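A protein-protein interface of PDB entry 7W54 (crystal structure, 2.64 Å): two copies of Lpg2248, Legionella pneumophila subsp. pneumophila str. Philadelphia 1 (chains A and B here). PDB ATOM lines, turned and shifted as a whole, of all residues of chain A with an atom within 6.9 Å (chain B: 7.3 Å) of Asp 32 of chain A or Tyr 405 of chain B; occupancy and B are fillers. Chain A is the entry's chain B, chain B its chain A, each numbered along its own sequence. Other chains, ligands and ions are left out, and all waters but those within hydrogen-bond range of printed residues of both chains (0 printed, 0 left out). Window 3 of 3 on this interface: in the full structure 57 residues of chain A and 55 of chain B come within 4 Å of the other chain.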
ATOM      1  N   GLU A  25      -2.053   5.097   6.769  1.00  0.00           N
ATOM      2  CA  GLU A  25      -2.951   4.083   6.220  1.00  0.00           C
ATOM      3  C   GLU A  25      -2.287   3.274   5.110  1.00  0.00           C
ATOM      4  O   GLU A  25      -2.540   2.069   4.981  1.00  0.00           O
ATOM      5  CB  GLU A  25      -4.238   4.739   5.722  1.00  0.00           C
ATOM      6  CG  GLU A  25      -5.137   5.242   6.838  1.00  0.00           C
ATOM      7  CD  GLU A  25      -5.657   4.120   7.720  1.00  0.00           C
ATOM      8  OE1 GLU A  25      -5.764   2.974   7.230  1.00  0.00           O
ATOM      9  OE2 GLU A  25      -5.963   4.382   8.902  1.00  0.00           O
ATOM     10  N   ILE A  26      -1.442   3.909   4.295  1.00  0.00           N
ATOM     11  CA  ILE A  26      -0.742   3.180   3.241  1.00  0.00           C
ATOM     12  C   ILE A  26       0.311   2.256   3.841  1.00  0.00           C
ATOM     13  O   ILE A  26       0.439   1.094   3.440  1.00  0.00           O
ATOM     14  CB  ILE A  26      -0.120   4.158   2.226  1.00  0.00           C
ATOM     15  CG1 ILE A  26      -1.204   4.799   1.355  1.00  0.00           C
ATOM     16  CG2 ILE A  26       0.905   3.447   1.354  1.00  0.00           C
ATOM     17  CD1 ILE A  26      -0.702   5.951   0.511  1.00  0.00           C
ATOM     18  N   LEU A  27       1.075   2.753   4.817  1.00  0.00           N
ATOM     19  CA  LEU A  27       2.108   1.920   5.421  1.00  0.00           C
ATOM     20  C   LEU A  27       1.511   0.774   6.231  1.00  0.00           C
ATOM     21  O   LEU A  27       2.105  -0.308   6.295  1.00  0.00           O
ATOM     22  CB  LEU A  27       3.026   2.776   6.294  1.00  0.00           C
ATOM     23  CG  LEU A  27       3.918   3.759   5.530  1.00  0.00           C
ATOM     24  CD1 LEU A  27       4.940   4.403   6.456  1.00  0.00           C
ATOM     25  CD2 LEU A  27       4.611   3.071   4.365  1.00  0.00           C
ATOM     26  N   SER A  28       0.341   0.978   6.839  1.00  0.00           N
ATOM     27  CA  SER A  28      -0.273  -0.081   7.635  1.00  0.00           C
ATOM     28  C   SER A  28      -0.651  -1.297   6.801  1.00  0.00           C
ATOM     29  O   SER A  28      -0.775  -2.397   7.351  1.00  0.00           O
ATOM     30  CB  SER A  28      -1.515   0.450   8.349  1.00  0.00           C
ATOM     31  OG  SER A  28      -2.577   0.651   7.432  1.00  0.00           O
ATOM     32  N   GLY A  29      -0.840  -1.127   5.494  1.00  0.00           N
ATOM     33  CA  GLY A  29      -1.288  -2.195   4.629  1.00  0.00           C
ATOM     34  C   GLY A  29      -2.781  -2.227   4.387  1.00  0.00           C
ATOM     35  O   GLY A  29      -3.224  -2.908   3.454  1.00  0.00           O
ATOM     36  N   ARG A  30      -3.566  -1.495   5.180  1.00  0.00           N
ATOM     37  CA  ARG A  30      -5.022  -1.518   5.083  1.00  0.00           C
ATOM     38  C   ARG A  30      -5.556  -0.933   3.779  1.00  0.00           C
ATOM     39  O   ARG A  30      -6.773  -0.968   3.568  1.00  0.00           O
ATOM     40  CB  ARG A  30      -5.635  -0.769   6.269  1.00  0.00           C
ATOM     41  CG  ARG A  30      -5.133  -1.239   7.624  1.00  0.00           C
ATOM     42  CD  ARG A  30      -5.996  -0.701   8.755  1.00  0.00           C
ATOM     43  NE  ARG A  30      -5.703   0.697   9.052  1.00  0.00           N
ATOM     44  CZ  ARG A  30      -4.760   1.098   9.898  1.00  0.00           C
ATOM     45  NH1 ARG A  30      -4.014   0.204  10.533  1.00  0.00           N
ATOM     46  NH2 ARG A  30      -4.564   2.392  10.112  1.00  0.00           N
ATOM     47  N   LEU A  31      -4.702  -0.399   2.906  1.00  0.00           N
ATOM     48  CA  LEU A  31      -5.145   0.150   1.630  1.00  0.00           C
ATOM     49  C   LEU A  31      -4.591  -0.613   0.435  1.00  0.00           C
ATOM     50  O   LEU A  31      -4.724  -0.143  -0.701  1.00  0.00           O
ATOM     51  CB  LEU A  31      -4.763   1.631   1.524  1.00  0.00           C
ATOM     52  CG  LEU A  31      -5.713   2.610   2.214  1.00  0.00           C
ATOM     53  CD1 LEU A  31      -5.101   4.001   2.272  1.00  0.00           C
ATOM     54  CD2 LEU A  31      -7.058   2.639   1.508  1.00  0.00           C
ATOM     55  N   ASP A  32      -3.977  -1.780   0.657  1.00  0.00           N
ATOM     56  CA  ASP A  32      -3.418  -2.544  -0.455  1.00  0.00           C
ATOM     57  C   ASP A  32      -4.502  -2.961  -1.442  1.00  0.00           C
ATOM     58  O   ASP A  32      -4.271  -2.983  -2.658  1.00  0.00           O
ATOM     59  CB  ASP A  32      -2.673  -3.769   0.078  1.00  0.00           C
ATOM     60  CG  ASP A  32      -1.381  -3.402   0.787  1.00  0.00           C
ATOM     61  OD1 ASP A  32      -1.026  -2.204   0.796  1.00  0.00           O
ATOM     62  OD2 ASP A  32      -0.722  -4.310   1.338  1.00  0.00           O
ATOM     63  N   SER A  33      -5.698  -3.277  -0.936  1.00  0.00           N
ATOM     64  CA  SER A  33      -6.797  -3.697  -1.800  1.00  0.00           C
ATOM     65  C   SER A  33      -7.156  -2.631  -2.826  1.00  0.00           C
ATOM     66  O   SER A  33      -7.607  -2.958  -3.929  1.00  0.00           O
ATOM     67  CB  SER A  33      -8.022  -4.041  -0.954  1.00  0.00           C
ATOM     68  OG  SER A  33      -8.221  -3.068   0.057  1.00  0.00           O
ATOM     69  N   GLN A  34      -6.967  -1.357  -2.485  1.00  0.00           N
ATOM     70  CA  GLN A  34      -7.280  -0.253  -3.381  1.00  0.00           C
ATOM     71  C   GLN A  34      -6.117   0.117  -4.290  1.00  0.00           C
ATOM     72  O   GLN A  34      -6.202   1.125  -5.000  1.00  0.00           O
ATOM     73  CB  GLN A  34      -7.715   0.972  -2.575  1.00  0.00           C
ATOM     74  CG  GLN A  34      -8.682   0.655  -1.450  1.00  0.00           C
ATOM     75  CD  GLN A  34      -9.975   0.046  -1.954  1.00  0.00           C
ATOM     76  OE1 GLN A  34     -10.860   0.754  -2.434  1.00  0.00           O
ATOM     77  NE2 GLN A  34     -10.092  -1.273  -1.846  1.00  0.00           N
ATOM     78  N   LEU A  35      -5.041  -0.675  -4.282  1.00  0.00           N
ATOM     79  CA  LEU A  35      -3.883  -0.404  -5.132  1.00  0.00           C
ATOM     80  C   LEU A  35      -4.288  -0.189  -6.587  1.00  0.00           C
ATOM     81  O   LEU A  35      -3.746   0.687  -7.269  1.00  0.00           O
ATOM     82  CB  LEU A  35      -2.897  -1.566  -5.012  1.00  0.00           C
ATOM     83  CG  LEU A  35      -1.476  -1.500  -5.572  1.00  0.00           C
ATOM     84  CD1 LEU A  35      -0.679  -2.617  -4.944  1.00  0.00           C
ATOM     85  CD2 LEU A  35      -1.440  -1.635  -7.081  1.00  0.00           C
ATOM     86  N   ASP A  36      -5.239  -0.981  -7.076  1.00  0.00           N
ATOM     87  CA  ASP A  36      -5.618  -0.978  -8.483  1.00  0.00           C
ATOM     88  C   ASP A  36      -6.675   0.065  -8.822  1.00  0.00           C
ATOM     89  O   ASP A  36      -6.875   0.362 -10.005  1.00  0.00           O
ATOM     90  CB  ASP A  36      -6.133  -2.367  -8.881  1.00  0.00           C
ATOM     91  CG  ASP A  36      -5.980  -2.654 -10.365  1.00  0.00           C
ATOM     92  OD1 ASP A  36      -5.678  -1.720 -11.137  1.00  0.00           O
ATOM     93  OD2 ASP A  36      -6.163  -3.825 -10.762  1.00  0.00           O
ATOM     94  N   SER A  58       5.517   2.764  -8.478  1.00  0.00           N
ATOM     95  CA  SER A  58       4.602   1.795  -7.960  1.00  0.00           C
ATOM     96  C   SER A  58       4.335   1.918  -6.497  1.00  0.00           C
ATOM     97  O   SER A  58       4.893   2.744  -5.825  1.00  0.00           O
ATOM     98  CB  SER A  58       5.201   0.440  -8.179  1.00  0.00           C
ATOM     99  OG  SER A  58       6.317   0.300  -7.355  1.00  0.00           O
ATOM    100  N   TRP A  59       3.484   1.026  -6.029  1.00  0.00           N
ATOM    101  CA  TRP A  59       3.058   0.937  -4.659  1.00  0.00           C
ATOM    102  C   TRP A  59       4.176   0.538  -3.773  1.00  0.00           C
ATOM    103  O   TRP A  59       4.269   1.010  -2.683  1.00  0.00           O
ATOM    104  CB  TRP A  59       1.981  -0.111  -4.563  1.00  0.00           C
ATOM    105  CG  TRP A  59       1.176  -0.098  -3.345  1.00  0.00           C
ATOM    106  CD1 TRP A  59       1.133  -1.052  -2.407  1.00  0.00           C
ATOM    107  CD2 TRP A  59       0.254   0.895  -2.947  1.00  0.00           C
ATOM    108  NE1 TRP A  59       0.251  -0.721  -1.439  1.00  0.00           N
ATOM    109  CE2 TRP A  59      -0.307   0.479  -1.753  1.00  0.00           C
ATOM    110  CE3 TRP A  59      -0.149   2.102  -3.486  1.00  0.00           C
ATOM    111  CZ2 TRP A  59      -1.236   1.216  -1.092  1.00  0.00           C
ATOM    112  CZ3 TRP A  59      -1.071   2.831  -2.827  1.00  0.00           C
ATOM    113  CH2 TRP A  59      -1.608   2.393  -1.646  1.00  0.00           C
ATOM    114  N   LYS A  60       5.026  -0.355  -4.230  1.00  0.00           N
ATOM    115  CA  LYS A  60       6.148  -0.779  -3.400  1.00  0.00           C
ATOM    116  C   LYS A  60       7.088   0.380  -3.099  1.00  0.00           C
ATOM    117  O   LYS A  60       7.534   0.550  -1.958  1.00  0.00           O
ATOM    118  CB  LYS A  60       6.906  -1.915  -4.084  1.00  0.00           C
ATOM    119  CG  LYS A  60       8.014  -2.515  -3.235  1.00  0.00           C
ATOM    120  CD  LYS A  60       8.817  -3.545  -4.011  1.00  0.00           C
ATOM    121  CE  LYS A  60      10.235  -3.065  -4.250  1.00  0.00           C
ATOM    122  NZ  LYS A  60      11.201  -3.768  -3.370  1.00  0.00           N
ATOM    123  N   THR A  61       7.399   1.193  -4.106  1.00  0.00           N
ATOM    124  CA  THR A  61       8.327   2.292  -3.892  1.00  0.00           C
ATOM    125  C   THR A  61       7.660   3.512  -3.278  1.00  0.00           C
ATOM    126  O   THR A  61       8.350   4.331  -2.665  1.00  0.00           O
ATOM    127  CB  THR A  61       9.013   2.652  -5.205  1.00  0.00           C
ATOM    128  OG1 THR A  61       8.124   3.415  -6.025  1.00  0.00           O
ATOM    129  CG2 THR A  61       9.383   1.381  -5.919  1.00  0.00           C
ATOM    130  N   LYS A  63       5.544   3.013  -0.775  1.00  0.00           N
ATOM    131  CA  LYS A  63       5.778   2.568   0.594  1.00  0.00           C
ATOM    132  C   LYS A  63       7.235   2.753   0.995  1.00  0.00           C
ATOM    133  O   LYS A  63       7.530   3.087   2.148  1.00  0.00           O
ATOM    134  CB  LYS A  63       5.367   1.106   0.752  1.00  0.00           C
ATOM    135  CG  LYS A  63       3.877   0.895   0.908  1.00  0.00           C
ATOM    136  CD  LYS A  63       3.569  -0.551   1.246  1.00  0.00           C
ATOM    137  CE  LYS A  63       2.077  -0.776   1.394  1.00  0.00           C
ATOM    138  NZ  LYS A  63       1.771  -2.179   1.779  1.00  0.00           N
ATOM    139  N   ALA B 401      10.180  -8.083  -8.397  1.00  0.00           N
ATOM    140  CA  ALA B 401       9.516  -7.615  -7.188  1.00  0.00           C
ATOM    141  C   ALA B 401       8.206  -6.903  -7.484  1.00  0.00           C
ATOM    142  O   ALA B 401       7.374  -6.767  -6.579  1.00  0.00           O
ATOM    143  CB  ALA B 401      10.449  -6.689  -6.409  1.00  0.00           C
ATOM    144  N   ALA B 402       8.000  -6.448  -8.724  1.00  0.00           N
ATOM    145  CA  ALA B 402       6.724  -5.840  -9.086  1.00  0.00           C
ATOM    146  C   ALA B 402       5.552  -6.798  -8.907  1.00  0.00           C
ATOM    147  O   ALA B 402       4.401  -6.350  -8.856  1.00  0.00           O
ATOM    148  CB  ALA B 402       6.774  -5.339 -10.532  1.00  0.00           C
ATOM    149  N   LEU B 403       5.817  -8.102  -8.799  1.00  0.00           N
ATOM    150  CA  LEU B 403       4.750  -9.088  -8.678  1.00  0.00           C
ATOM    151  C   LEU B 403       4.190  -9.187  -7.265  1.00  0.00           C
ATOM    152  O   LEU B 403       3.083  -9.708  -7.093  1.00  0.00           O
ATOM    153  CB  LEU B 403       5.247 -10.468  -9.119  1.00  0.00           C
ATOM    154  CG  LEU B 403       5.245 -10.883 -10.593  1.00  0.00           C
ATOM    155  CD1 LEU B 403       5.872  -9.827 -11.484  1.00  0.00           C
ATOM    156  CD2 LEU B 403       5.974 -12.205 -10.752  1.00  0.00           C
ATOM    157  N   TYR B 404       4.926  -8.714  -6.256  1.00  0.00           N
ATOM    158  CA  TYR B 404       4.471  -8.781  -4.871  1.00  0.00           C
ATOM    159  C   TYR B 404       3.169  -8.007  -4.699  1.00  0.00           C
ATOM    160  O   TYR B 404       2.114  -8.603  -4.461  1.00  0.00           O
ATOM    161  CB  TYR B 404       5.551  -8.248  -3.928  1.00  0.00           C
ATOM    162  CG  TYR B 404       5.203  -8.362  -2.461  1.00  0.00           C
ATOM    163  CD1 TYR B 404       5.339  -9.569  -1.787  1.00  0.00           C
ATOM    164  CD2 TYR B 404       4.747  -7.262  -1.747  1.00  0.00           C
ATOM    165  CE1 TYR B 404       5.024  -9.679  -0.443  1.00  0.00           C
ATOM    166  CE2 TYR B 404       4.432  -7.361  -0.404  1.00  0.00           C
ATOM    167  CZ  TYR B 404       4.572  -8.570   0.242  1.00  0.00           C
ATOM    168  OH  TYR B 404       4.261  -8.666   1.577  1.00  0.00           O
ATOM    169  N   TYR B 405       3.235  -6.681  -4.807  1.00  0.00           N
ATOM    170  CA  TYR B 405       2.039  -5.858  -4.978  1.00  0.00           C
ATOM    171  C   TYR B 405       1.721  -5.849  -6.467  1.00  0.00           C
ATOM    172  O   TYR B 405       2.281  -5.058  -7.229  1.00  0.00           O
ATOM    173  CB  TYR B 405       2.263  -4.443  -4.457  1.00  0.00           C
ATOM    174  CG  TYR B 405       2.717  -4.343  -3.020  1.00  0.00           C
ATOM    175  CD1 TYR B 405       1.909  -4.775  -1.978  1.00  0.00           C
ATOM    176  CD2 TYR B 405       3.952  -3.791  -2.705  1.00  0.00           C
ATOM    177  CE1 TYR B 405       2.323  -4.672  -0.660  1.00  0.00           C
ATOM    178  CE2 TYR B 405       4.377  -3.685  -1.394  1.00  0.00           C
ATOM    179  CZ  TYR B 405       3.560  -4.125  -0.376  1.00  0.00           C
ATOM    180  OH  TYR B 405       3.983  -4.018   0.929  1.00  0.00           O
ATOM    181  N   GLY B 406       0.824  -6.730  -6.891  1.00  0.00           N
ATOM    182  CA  GLY B 406       0.681  -7.011  -8.308  1.00  0.00           C
ATOM    183  C   GLY B 406      -0.135  -6.037  -9.135  1.00  0.00           C
ATOM    184  O   GLY B 406      -1.180  -6.414  -9.675  1.00  0.00           O
ATOM    185  N   ASP B 407       0.326  -4.798  -9.269  1.00  0.00           N
ATOM    186  CA  ASP B 407      -0.328  -3.852 -10.163  1.00  0.00           C
ATOM    187  C   ASP B 407      -0.211  -4.360 -11.596  1.00  0.00           C
ATOM    188  O   ASP B 407       0.910  -4.610 -12.065  1.00  0.00           O
ATOM    189  CB  ASP B 407       0.296  -2.461 -10.040  1.00  0.00           C
ATOM    190  CG  ASP B 407      -0.329  -1.431 -10.993  1.00  0.00           C
ATOM    191  OD1 ASP B 407      -1.339  -1.716 -11.670  1.00  0.00           O
ATOM    192  OD2 ASP B 407       0.204  -0.296 -11.022  1.00  0.00           O
ATOM    193  N   PRO B 408      -1.322  -4.529 -12.317  1.00  0.00           N
ATOM    194  CA  PRO B 408      -1.247  -5.044 -13.695  1.00  0.00           C
ATOM    195  C   PRO B 408      -0.317  -4.274 -14.618  1.00  0.00           C
ATOM    196  O   PRO B 408       0.292  -4.892 -15.500  1.00  0.00           O
ATOM    197  CB  PRO B 408      -2.703  -4.954 -14.163  1.00  0.00           C
ATOM    198  CG  PRO B 408      -3.502  -5.136 -12.918  1.00  0.00           C
ATOM    199  CD  PRO B 408      -2.707  -4.482 -11.813  1.00  0.00           C
ATOM    200  N   ASP B 410       2.568  -3.136 -14.189  1.00  0.00           N
ATOM    201  CA  ASP B 410       3.929  -3.632 -14.045  1.00  0.00           C
ATOM    202  C   ASP B 410       4.058  -5.114 -14.377  1.00  0.00           C
ATOM    203  O   ASP B 410       5.175  -5.641 -14.369  1.00  0.00           O
ATOM    204  CB  ASP B 410       4.434  -3.381 -12.619  1.00  0.00           C
ATOM    205  CG  ASP B 410       4.878  -1.948 -12.399  1.00  0.00           C
ATOM    206  OD1 ASP B 410       4.356  -1.049 -13.090  1.00  0.00           O
ATOM    207  OD2 ASP B 410       5.748  -1.720 -11.531  1.00  0.00           O
ATOM    208  N   THR B 411       2.948  -5.797 -14.665  1.00  0.00           N
ATOM    209  CA  THR B 411       2.964  -7.224 -14.968  1.00  0.00           C
ATOM    210  C   THR B 411       2.483  -7.518 -16.385  1.00  0.00           C
ATOM    211  O   THR B 411       1.996  -8.622 -16.652  1.00  0.00           O
ATOM    212  CB  THR B 411       2.121  -8.001 -13.956  1.00  0.00           C
ATOM    213  OG1 THR B 411       0.944  -7.252 -13.635  1.00  0.00           O
ATOM    214  CG2 THR B 411       2.907  -8.243 -12.684  1.00  0.00           C
ATOM    215  N   MET B 428       5.490 -16.034  -4.041  1.00  0.00           N
ATOM    216  CA  MET B 428       5.057 -14.666  -3.793  1.00  0.00           C
ATOM    217  C   MET B 428       3.798 -14.576  -2.929  1.00  0.00           C
ATOM    218  O   MET B 428       3.797 -13.923  -1.883  1.00  0.00           O
ATOM    219  CB  MET B 428       4.809 -13.968  -5.134  1.00  0.00           C
ATOM    220  CG  MET B 428       5.085 -12.477  -5.151  1.00  0.00           C
ATOM    221  SD  MET B 428       6.983 -12.067  -4.998  1.00  0.00           S
ATOM    222  CE  MET B 428       7.447 -11.966  -6.878  1.00  0.00           C
ATOM    223  N   ARG B 433       2.645 -11.795   4.954  1.00  0.00           N
ATOM    224  CA  ARG B 433       2.817 -10.393   4.725  1.00  0.00           C
ATOM    225  C   ARG B 433       2.827  -9.622   6.018  1.00  0.00           C
ATOM    226  O   ARG B 433       3.273  -8.487   6.041  1.00  0.00           O
ATOM    227  CB  ARG B 433       1.732  -9.890   3.783  1.00  0.00           C
ATOM    228  CG  ARG B 433       1.509 -10.788   2.577  1.00  0.00           C
ATOM    229  CD  ARG B 433       1.151 -10.008   1.324  1.00  0.00           C
ATOM    230  NE  ARG B 433       1.585 -10.702   0.116  1.00  0.00           N
ATOM    231  CZ  ARG B 433       1.566 -10.169  -1.101  1.00  0.00           C
ATOM    232  NH1 ARG B 433       1.139  -8.929  -1.279  1.00  0.00           N
ATOM    233  NH2 ARG B 433       1.983 -10.875  -2.139  1.00  0.00           N
ATOM    234  N   VAL B 436       6.258  -8.957   6.910  1.00  0.00           N
ATOM    235  CA  VAL B 436       6.898  -7.953   6.069  1.00  0.00           C
ATOM    236  C   VAL B 436       6.794  -6.598   6.751  1.00  0.00           C
ATOM    237  O   VAL B 436       5.704  -6.169   7.148  1.00  0.00           O
ATOM    238  CB  VAL B 436       6.254  -7.917   4.673  1.00  0.00           C
ATOM    239  CG1 VAL B 436       6.695  -6.673   3.916  1.00  0.00           C
ATOM    240  CG2 VAL B 436       6.602  -9.172   3.891  1.00  0.00           C
ATOM    241  N   HIS B 437       7.925  -5.924   6.896  1.00  0.00           N
ATOM    242  CA  HIS B 437       7.901  -4.546   7.364  1.00  0.00           C
ATOM    243  C   HIS B 437       7.600  -3.618   6.191  1.00  0.00           C
ATOM    244  O   HIS B 437       8.278  -3.696   5.161  1.00  0.00           O
ATOM    245  CB  HIS B 437       9.229  -4.172   8.015  1.00  0.00           C
ATOM    246  CG  HIS B 437       9.355  -4.626   9.437  1.00  0.00           C
ATOM    247  ND1 HIS B 437       9.788  -5.889   9.781  1.00  0.00           N
ATOM    248  CD2 HIS B 437       9.105  -3.984  10.603  1.00  0.00           C
ATOM    249  CE1 HIS B 437       9.799  -6.005  11.097  1.00  0.00           C
ATOM    250  NE2 HIS B 437       9.390  -4.863  11.619  1.00  0.00           N
ATOM    251  N   PRO B 438       6.583  -2.762   6.295  1.00  0.00           N
ATOM    252  CA  PRO B 438       6.233  -1.885   5.168  1.00  0.00           C
ATOM    253  C   PRO B 438       7.400  -0.998   4.764  1.00  0.00           C
ATOM    254  O   PRO B 438       8.178  -0.540   5.603  1.00  0.00           O
ATOM    255  CB  PRO B 438       5.059  -1.057   5.705  1.00  0.00           C
ATOM    256  CG  PRO B 438       4.980  -1.349   7.178  1.00  0.00           C
ATOM    257  CD  PRO B 438       5.615  -2.675   7.399  1.00  0.00           C
ATOM    258  N   GLY B 439       7.514  -0.757   3.460  1.00  0.00           N
ATOM    259  CA  GLY B 439       8.680  -0.092   2.919  1.00  0.00           C
ATOM    260  C   GLY B 439       9.961  -0.885   3.020  1.00  0.00           C
ATOM    261  O   GLY B 439      11.014  -0.386   2.609  1.00  0.00           O
ATOM    262  N   HIS B 440       9.906  -2.104   3.562  1.00  0.00           N
ATOM    263  CA  HIS B 440      11.055  -2.989   3.693  1.00  0.00           C
ATOM    264  C   HIS B 440      10.743  -4.358   3.102  1.00  0.00           C
ATOM    265  O   HIS B 440      11.269  -5.376   3.561  1.00  0.00           O
ATOM    266  CB  HIS B 440      11.484  -3.116   5.155  1.00  0.00           C
ATOM    267  CG  HIS B 440      12.058  -1.857   5.722  1.00  0.00           C
ATOM    268  ND1 HIS B 440      11.304  -0.950   6.437  1.00  0.00           N
ATOM    269  CD2 HIS B 440      13.311  -1.347   5.671  1.00  0.00           C
ATOM    270  CE1 HIS B 440      12.069   0.062   6.805  1.00  0.00           C
ATOM    271  NE2 HIS B 440      13.291  -0.155   6.353  1.00  0.00           N
ATOM    272  N   GLU B 441       9.872  -4.389   2.091  1.00  0.00           N
ATOM    273  CA  GLU B 441       9.571  -5.630   1.390  1.00  0.00           C
ATOM    274  C   GLU B 441      10.835  -6.281   0.848  1.00  0.00           C
ATOM    275  O   GLU B 441      10.917  -7.514   0.763  1.00  0.00           O
ATOM    276  CB  GLU B 441       8.583  -5.352   0.254  1.00  0.00           C
ATOM    277  CG  GLU B 441       7.248  -4.755   0.704  1.00  0.00           C
ATOM    278  CD  GLU B 441       7.303  -3.250   0.915  1.00  0.00           C
ATOM    279  OE1 GLU B 441       8.419  -2.688   0.958  1.00  0.00           O
ATOM    280  OE2 GLU B 441       6.227  -2.628   1.041  1.00  0.00           O
ATOM    281  N   LEU B 445      12.208  -9.994  -0.099  1.00  0.00           N
ATOM    282  CA  LEU B 445      12.228 -10.262  -1.532  1.00  0.00           C
ATOM    283  C   LEU B 445      13.615 -10.624  -2.054  1.00  0.00           C
ATOM    284  O   LEU B 445      13.722 -11.456  -2.962  1.00  0.00           O
ATOM    285  CB  LEU B 445      11.674  -9.060  -2.295  1.00  0.00           C
ATOM    286  CG  LEU B 445      10.148  -8.963  -2.255  1.00  0.00           C
ATOM    287  CD1 LEU B 445       9.655  -7.778  -3.059  1.00  0.00           C
ATOM    288  CD2 LEU B 445       9.516 -10.256  -2.757  1.00  0.00           C
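Among the printed residues, merely in contact across the chains: Leu 27 of chain A with Pro 438 of chain B (3.1 Å), Asp 32 of chain A with Tyr 405 of chain B (3.7 Å), Leu 35 of chain A with Tyr 405 of chain B (3.5 Å), Leu 35 of chain A with Asp 407 of chain B (3.5 Å), Asp 36 of chain A with Pro 408 of chain B (3.7 Å), Trp 59 of chain A with Tyr 405 of chain B (3.7 Å), Lys 60 of chain A with Tyr 405 of chain B (3.8 Å), Lys 63 of chain A with Gly 439 of chain B (3.5 Å) and Lys 63 of chain A with Glu 441 of chain B (3.4 Å).
Of the printed residues of chain B, Asp 32 of chain A touches Tyr 405. Of chain A, only Asp 32, Leu 35, Trp 59, Lys 60 and Lys 63 come within 4 Å of Tyr 405 of chain B. Of the printed residues of chain A, Pro 408 of chain B touches Asp 36. Of the printed residues of chain B, Lys 60 of chain A touches Tyr 405 (3.8 Å). Of the printed residues of chain B, Leu 35 of chain A touches Tyr 405 and Asp 407. Printed residues of chain B within 4 Å of Lys 63 of chain A: Tyr 405, Gly 439 and Glu 441. The nearest residue of chain B that does not touch Asp 32 of chain A is Arg 433 of chain B (5.6 Å). The nearest printed residue of chain B that does not touch Leu 35 of chain A is Gly 406 of chain B (4.8 Å).
Hydrophobic or aromatic side chains of chain A that line the printed part of chain B: Leu 35 and Trp 59. Hydrophobic or aromatic side chains of chain B that line the printed part of chain A: Tyr 405, Pro 408 and Pro 438. Among the printed residues, no Asp or Glu carboxylate lies within 4 Å of a Lys or Arg side-chain nitrogen of the other chain.
The backbone carbonyl oxygen of Pro 438 of chain B is in hydrogen-bond range of a ring nitrogen (ND1) of His 440 of chain B (3.3 Å). OG of Ser 58 of chain A lies close to N of Lys 60 of chain A (3.4 Å). OD1 of Asp 32 of chain A sits at hydrogen-bond distance from NE1 of Trp 59 of chain A. The backbone NH of Gly 439 of chain B sits close to the side-chain carboxylate of Glu 441 of chain B (3.3 Å). The side-chain carboxylate of Glu 441 of chain B sits at hydrogen-bond distance from the side-chain hydroxyl of Tyr 405 of chain B, at 2.6 Å. The backbone carbonyl oxygen of Asp 407 of chain B lies within hydrogen-bond range of the side-chain hydroxyl of Thr 411 of chain B (3.1 Å).
OH of Tyr 405 of chain B lies within hydrogen-bond range of NZ of Lys 63 of chain A.
No position is printed for both chains. Of the 10 pairs that touch across the chains among the printed residues, none has its exchanged pair printed and touching as well.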
